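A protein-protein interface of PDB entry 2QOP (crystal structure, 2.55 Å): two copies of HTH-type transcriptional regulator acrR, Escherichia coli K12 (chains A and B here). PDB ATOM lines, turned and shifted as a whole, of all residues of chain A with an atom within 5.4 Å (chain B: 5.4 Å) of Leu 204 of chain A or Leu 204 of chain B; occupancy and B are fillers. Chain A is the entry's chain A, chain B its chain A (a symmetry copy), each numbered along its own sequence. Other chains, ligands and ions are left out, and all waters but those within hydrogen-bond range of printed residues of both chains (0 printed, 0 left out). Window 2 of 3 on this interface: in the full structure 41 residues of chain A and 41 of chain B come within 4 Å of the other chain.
Glu 200 of chain A touches Cys 205 of chain B, and with the chains exchanged Cys 205 of chain A touches Glu 200 of chain B.
Met 201 of chain A touches its own counterpart, Met 201 of chain B.
Leu 204 of chain B touches its own counterpart, Leu 204 of chain A.
Cys 205 of chain B touches its own counterpart, Cys 205 of chain A.
Positions printed for both chains: 200, 201, 202, 203, 204, 205, 206 and 209.
Of the 9 pairs that touch across the chains among the printed residues, 9 have their exchanged pair printed and touching as well.
Cys 205 of chain B touches Met 201 of chain A.
Leu 204 of chain B touches Leu 204 of chain A (O to CD2, 3.4 Å).
Met 201 of chain B touches Cys 205 of chain A (N to SG, 3.9 Å).
The side-chain sulfur (SG) of Cys 205 of chain B lies within hydrogen-bond range of the backbone carbonyl oxygen (O) of Glu 200 of chain A.
SG of Cys 205 of chain A is in hydrogen-bond range of O of Glu 200 of chain B (3.4 Å).
The side-chain sulfur of Cys 205 of chain B lies within hydrogen-bond range of the side-chain sulfur of Cys 205 of chain A, at 3.7 Å.
The side-chain carboxylate of Glu 200 of chain A sits close to the backbone carbonyl oxygen of Pro 206 of chain B, at 3.1 Å.
The side-chain sulfur of Met 201 of chain A sits close to the side-chain sulfur of Met 201 of chain B, at 3.7 Å.
The backbone carbonyl oxygen (O) of Pro 206 of chain A lies close to the side-chain carboxylate (OE1) of Glu 200 of chain B (3.1 Å).
Of the 8 printed residues of chain A, 5 touch a printed residue of chain B.
Along chain A the printed residues that touch a printed residue of chain B span positions 200 to 206.
Of the 8 printed residues of chain B, 5 touch a printed residue of chain A.
Hydrophobic or aromatic side chains of chain B that line the printed part of chain A: Met 201, Leu 204 and Pro 206.
Among the printed residues, no Asp or Glu carboxylate lies within 4 Å of a Lys or Arg side-chain nitrogen of the other chain.
Of the printed residues of chain B, Leu 204 of chain A touches Leu 204 (3.4 Å).
Leu 204 of chain B touches just one residue of chain A: Leu 204 (3.4 Å).
Of the printed residues of chain A, Met 201 of chain B touches Met 201 and Cys 205.
Printed residues of chain B within 4 Å of Glu 200 of chain A: Cys 205 and Pro 206.
Printed residues of chain B within 4 Å of Cys 205 of chain A: Glu 200 (3.4 Å), Met 201 (3.9 Å) and Cys 205 (3.7 Å).
Of the printed residues of chain A, Pro 206 of chain B touches Glu 200.
Tyr 202 of chain A touches none of the printed residues of chain B.
The nearest residue of chain B that does not touch Leu 204 of chain A is Pro 206 of chain B (4.2 Å).
The nearest printed residue of chain A that does not touch Met 201 of chain B is Glu 200 of chain A (6.9 Å).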
ATOM      1  N   GLU A 200      21.516  -9.333 -15.903  1.00  0.00           N
ATOM      2  CA  GLU A 200      20.921  -9.801 -14.648  1.00  0.00           C
ATOM      3  C   GLU A 200      21.108 -11.303 -14.412  1.00  0.00           C
ATOM      4  O   GLU A 200      20.863 -11.796 -13.308  1.00  0.00           O
ATOM      5  CB  GLU A 200      19.439  -9.417 -14.577  1.00  0.00           C
ATOM      6  CG  GLU A 200      19.197  -7.946 -14.241  1.00  0.00           C
ATOM      7  CD  GLU A 200      17.817  -7.451 -14.648  1.00  0.00           C
ATOM      8  OE1 GLU A 200      17.176  -8.080 -15.519  1.00  0.00           O
ATOM      9  OE2 GLU A 200      17.374  -6.422 -14.097  1.00  0.00           O
ATOM     10  N   MET A 201      21.543 -12.017 -15.450  1.00  0.00           N
ATOM     11  CA  MET A 201      21.861 -13.441 -15.346  1.00  0.00           C
ATOM     12  C   MET A 201      23.112 -13.688 -14.509  1.00  0.00           C
ATOM     13  O   MET A 201      23.133 -14.579 -13.660  1.00  0.00           O
ATOM     14  CB  MET A 201      22.058 -14.054 -16.735  1.00  0.00           C
ATOM     15  CG  MET A 201      20.781 -14.495 -17.423  1.00  0.00           C
ATOM     16  SD  MET A 201      21.095 -15.635 -18.788  1.00  0.00           S
ATOM     17  CE  MET A 201      21.679 -14.520 -20.061  1.00  0.00           C
ATOM     18  N   TYR A 202      24.147 -12.886 -14.752  1.00  0.00           N
ATOM     19  CA  TYR A 202      25.459 -13.097 -14.142  1.00  0.00           C
ATOM     20  C   TYR A 202      25.526 -12.695 -12.668  1.00  0.00           C
ATOM     21  O   TYR A 202      26.399 -13.166 -11.934  1.00  0.00           O
ATOM     22  CB  TYR A 202      26.549 -12.366 -14.938  1.00  0.00           C
ATOM     23  CG  TYR A 202      26.509 -12.597 -16.437  1.00  0.00           C
ATOM     24  CD1 TYR A 202      26.486 -11.521 -17.323  1.00  0.00           C
ATOM     25  CD2 TYR A 202      26.492 -13.888 -16.969  1.00  0.00           C
ATOM     26  CE1 TYR A 202      26.452 -11.722 -18.699  1.00  0.00           C
ATOM     27  CE2 TYR A 202      26.451 -14.099 -18.345  1.00  0.00           C
ATOM     28  CZ  TYR A 202      26.433 -13.012 -19.203  1.00  0.00           C
ATOM     29  OH  TYR A 202      26.396 -13.216 -20.563  1.00  0.00           O
ATOM     30  N   LEU A 203      24.605 -11.834 -12.238  1.00  0.00           N
ATOM     31  CA  LEU A 203      24.611 -11.317 -10.866  1.00  0.00           C
ATOM     32  C   LEU A 203      23.487 -11.849  -9.964  1.00  0.00           C
ATOM     33  O   LEU A 203      23.433 -11.517  -8.777  1.00  0.00           O
ATOM     34  CB  LEU A 203      24.657  -9.777 -10.856  1.00  0.00           C
ATOM     35  CG  LEU A 203      23.798  -8.949 -11.820  1.00  0.00           C
ATOM     36  CD1 LEU A 203      22.390  -8.739 -11.287  1.00  0.00           C
ATOM     37  CD2 LEU A 203      24.460  -7.606 -12.084  1.00  0.00           C
ATOM     38  N   LEU A 204      22.608 -12.681 -10.523  1.00  0.00           N
ATOM     39  CA  LEU A 204      21.513 -13.282  -9.753  1.00  0.00           C
ATOM     40  C   LEU A 204      21.390 -14.801  -9.909  1.00  0.00           C
ATOM     41  O   LEU A 204      21.307 -15.520  -8.911  1.00  0.00           O
ATOM     42  CB  LEU A 204      20.173 -12.605 -10.075  1.00  0.00           C
ATOM     43  CG  LEU A 204      19.529 -11.724  -8.996  1.00  0.00           C
ATOM     44  CD1 LEU A 204      20.256 -10.398  -8.812  1.00  0.00           C
ATOM     45  CD2 LEU A 204      18.064 -11.480  -9.320  1.00  0.00           C
ATOM     46  N   CYS A 205      21.383 -15.277 -11.154  1.00  0.00           N
ATOM     47  CA  CYS A 205      21.143 -16.693 -11.449  1.00  0.00           C
ATOM     48  C   CYS A 205      22.238 -17.628 -10.928  1.00  0.00           C
ATOM     49  O   CYS A 205      23.424 -17.389 -11.166  1.00  0.00           O
ATOM     50  CB  CYS A 205      20.944 -16.910 -12.953  1.00  0.00           C
ATOM     51  SG  CYS A 205      19.382 -16.283 -13.601  1.00  0.00           S
ATOM     52  N   PRO A 206      21.835 -18.693 -10.206  1.00  0.00           N
ATOM     53  CA  PRO A 206      22.732 -19.777  -9.792  1.00  0.00           C
ATOM     54  C   PRO A 206      23.203 -20.624 -10.980  1.00  0.00           C
ATOM     55  O   PRO A 206      23.010 -20.230 -12.133  1.00  0.00           O
ATOM     56  CB  PRO A 206      21.858 -20.617  -8.846  1.00  0.00           C
ATOM     57  CG  PRO A 206      20.693 -19.748  -8.498  1.00  0.00           C
ATOM     58  CD  PRO A 206      20.467 -18.905  -9.703  1.00  0.00           C
ATOM     59  N   ARG A 209      27.339 -19.884 -10.889  1.00  0.00           N
ATOM     60  CA  ARG A 209      28.238 -19.860  -9.740  1.00  0.00           C
ATOM     61  C   ARG A 209      28.812 -21.255  -9.505  1.00  0.00           C
ATOM     62  O   ARG A 209      28.190 -22.258  -9.865  1.00  0.00           O
ATOM     63  CB  ARG A 209      27.493 -19.392  -8.482  1.00  0.00           C
ATOM     64  CG  ARG A 209      26.555 -18.200  -8.676  1.00  0.00           C
ATOM     65  CD  ARG A 209      27.301 -16.871  -8.725  1.00  0.00           C
ATOM     66  NE  ARG A 209      26.380 -15.736  -8.769  1.00  0.00           N
ATOM     67  CZ  ARG A 209      25.896 -15.111  -7.697  1.00  0.00           C
ATOM     68  NH1 ARG A 209      26.241 -15.499  -6.475  1.00  0.00           N
ATOM     69  NH2 ARG A 209      25.064 -14.091  -7.848  1.00  0.00           N
ATOM     70  N   GLU B 200      16.081 -20.410 -14.436  1.00  0.00           N
ATOM     71  CA  GLU B 200      16.378 -19.485 -13.339  1.00  0.00           C
ATOM     72  C   GLU B 200      16.210 -18.012 -13.726  1.00  0.00           C
ATOM     73  O   GLU B 200      16.206 -17.135 -12.858  1.00  0.00           O
ATOM     74  CB  GLU B 200      17.781 -19.745 -12.779  1.00  0.00           C
ATOM     75  CG  GLU B 200      17.866 -20.975 -11.876  1.00  0.00           C
ATOM     76  CD  GLU B 200      19.279 -21.521 -11.728  1.00  0.00           C
ATOM     77  OE1 GLU B 200      20.139 -21.229 -12.587  1.00  0.00           O
ATOM     78  OE2 GLU B 200      19.528 -22.252 -10.746  1.00  0.00           O
ATOM     79  N   MET B 201      16.071 -17.753 -15.026  1.00  0.00           N
ATOM     80  CA  MET B 201      15.804 -16.407 -15.535  1.00  0.00           C
ATOM     81  C   MET B 201      14.401 -15.927 -15.174  1.00  0.00           C
ATOM     82  O   MET B 201      14.219 -14.788 -14.746  1.00  0.00           O
ATOM     83  CB  MET B 201      15.974 -16.360 -17.056  1.00  0.00           C
ATOM     84  CG  MET B 201      17.398 -16.145 -17.530  1.00  0.00           C
ATOM     85  SD  MET B 201      17.474 -15.605 -19.251  1.00  0.00           S
ATOM     86  CE  MET B 201      17.162 -17.137 -20.123  1.00  0.00           C
ATOM     87  N   TYR B 202      13.419 -16.810 -15.345  1.00  0.00           N
ATOM     88  CA  TYR B 202      12.010 -16.450 -15.190  1.00  0.00           C
ATOM     89  C   TYR B 202      11.573 -16.282 -13.733  1.00  0.00           C
ATOM     90  O   TYR B 202      10.573 -15.615 -13.458  1.00  0.00           O
ATOM     91  CB  TYR B 202      11.110 -17.473 -15.896  1.00  0.00           C
ATOM     92  CG  TYR B 202      11.519 -17.810 -17.317  1.00  0.00           C
ATOM     93  CD1 TYR B 202      11.704 -19.135 -17.711  1.00  0.00           C
ATOM     94  CD2 TYR B 202      11.724 -16.807 -18.268  1.00  0.00           C
ATOM     95  CE1 TYR B 202      12.076 -19.454 -19.012  1.00  0.00           C
ATOM     96  CE2 TYR B 202      12.103 -17.117 -19.571  1.00  0.00           C
ATOM     97  CZ  TYR B 202      12.276 -18.442 -19.936  1.00  0.00           C
ATOM     98  OH  TYR B 202      12.647 -18.753 -21.224  1.00  0.00           O
ATOM     99  N   LEU B 203      12.323 -16.879 -12.809  1.00  0.00           N
ATOM    100  CA  LEU B 203      11.964 -16.854 -11.387  1.00  0.00           C
ATOM    101  C   LEU B 203      12.862 -15.974 -10.505  1.00  0.00           C
ATOM    102  O   LEU B 203      12.615 -15.842  -9.303  1.00  0.00           O
ATOM    103  CB  LEU B 203      11.845 -18.281 -10.821  1.00  0.00           C
ATOM    104  CG  LEU B 203      12.871 -19.366 -11.175  1.00  0.00           C
ATOM    105  CD1 LEU B 203      14.098 -19.298 -10.281  1.00  0.00           C
ATOM    106  CD2 LEU B 203      12.230 -20.741 -11.075  1.00  0.00           C
ATOM    107  N   LEU B 204      13.887 -15.367 -11.103  1.00  0.00           N
ATOM    108  CA  LEU B 204      14.793 -14.474 -10.371  1.00  0.00           C
ATOM    109  C   LEU B 204      15.020 -13.116 -11.041  1.00  0.00           C
ATOM    110  O   LEU B 204      14.895 -12.077 -10.391  1.00  0.00           O
ATOM    111  CB  LEU B 204      16.138 -15.159 -10.088  1.00  0.00           C
ATOM    112  CG  LEU B 204      16.462 -15.549  -8.640  1.00  0.00           C
ATOM    113  CD1 LEU B 204      15.651 -16.746  -8.160  1.00  0.00           C
ATOM    114  CD2 LEU B 204      17.949 -15.827  -8.489  1.00  0.00           C
ATOM    115  N   CYS B 205      15.348 -13.133 -12.333  1.00  0.00           N
ATOM    116  CA  CYS B 205      15.717 -11.917 -13.064  1.00  0.00           C
ATOM    117  C   CYS B 205      14.574 -10.908 -13.203  1.00  0.00           C
ATOM    118  O   CYS B 205      13.470 -11.272 -13.614  1.00  0.00           O
ATOM    119  CB  CYS B 205      16.281 -12.261 -14.446  1.00  0.00           C
ATOM    120  SG  CYS B 205      17.922 -13.009 -14.422  1.00  0.00           S
ATOM    121  N   PRO B 206      14.841  -9.634 -12.852  1.00  0.00           N
ATOM    122  CA  PRO B 206      13.923  -8.516 -13.095  1.00  0.00           C
ATOM    123  C   PRO B 206      13.790  -8.191 -14.587  1.00  0.00           C
ATOM    124  O   PRO B 206      14.236  -8.973 -15.431  1.00  0.00           O
ATOM    125  CB  PRO B 206      14.583  -7.347 -12.346  1.00  0.00           C
ATOM    126  CG  PRO B 206      15.589  -7.971 -11.433  1.00  0.00           C
ATOM    127  CD  PRO B 206      16.057  -9.188 -12.149  1.00  0.00           C
ATOM    128  N   ARG B 209       9.724  -9.037 -15.224  1.00  0.00           N
ATOM    129  CA  ARG B 209       8.576  -8.677 -14.399  1.00  0.00           C
ATOM    130  C   ARG B 209       8.027  -7.322 -14.841  1.00  0.00           C
ATOM    131  O   ARG B 209       8.763  -6.495 -15.385  1.00  0.00           O
ATOM    132  CB  ARG B 209       8.974  -8.612 -12.918  1.00  0.00           C
ATOM    133  CG  ARG B 209       9.874  -9.747 -12.428  1.00  0.00           C
ATOM    134  CD  ARG B 209       9.101 -11.033 -12.160  1.00  0.00           C
ATOM    135  NE  ARG B 209       9.952 -12.060 -11.560  1.00  0.00           N
ATOM    136  CZ  ARG B 209      10.134 -12.223 -10.251  1.00  0.00           C
ATOM    137  NH1 ARG B 209       9.525 -11.427  -9.380  1.00  0.00           N
ATOM    138  NH2 ARG B 209      10.930 -13.186  -9.810  1.00  0.00           N
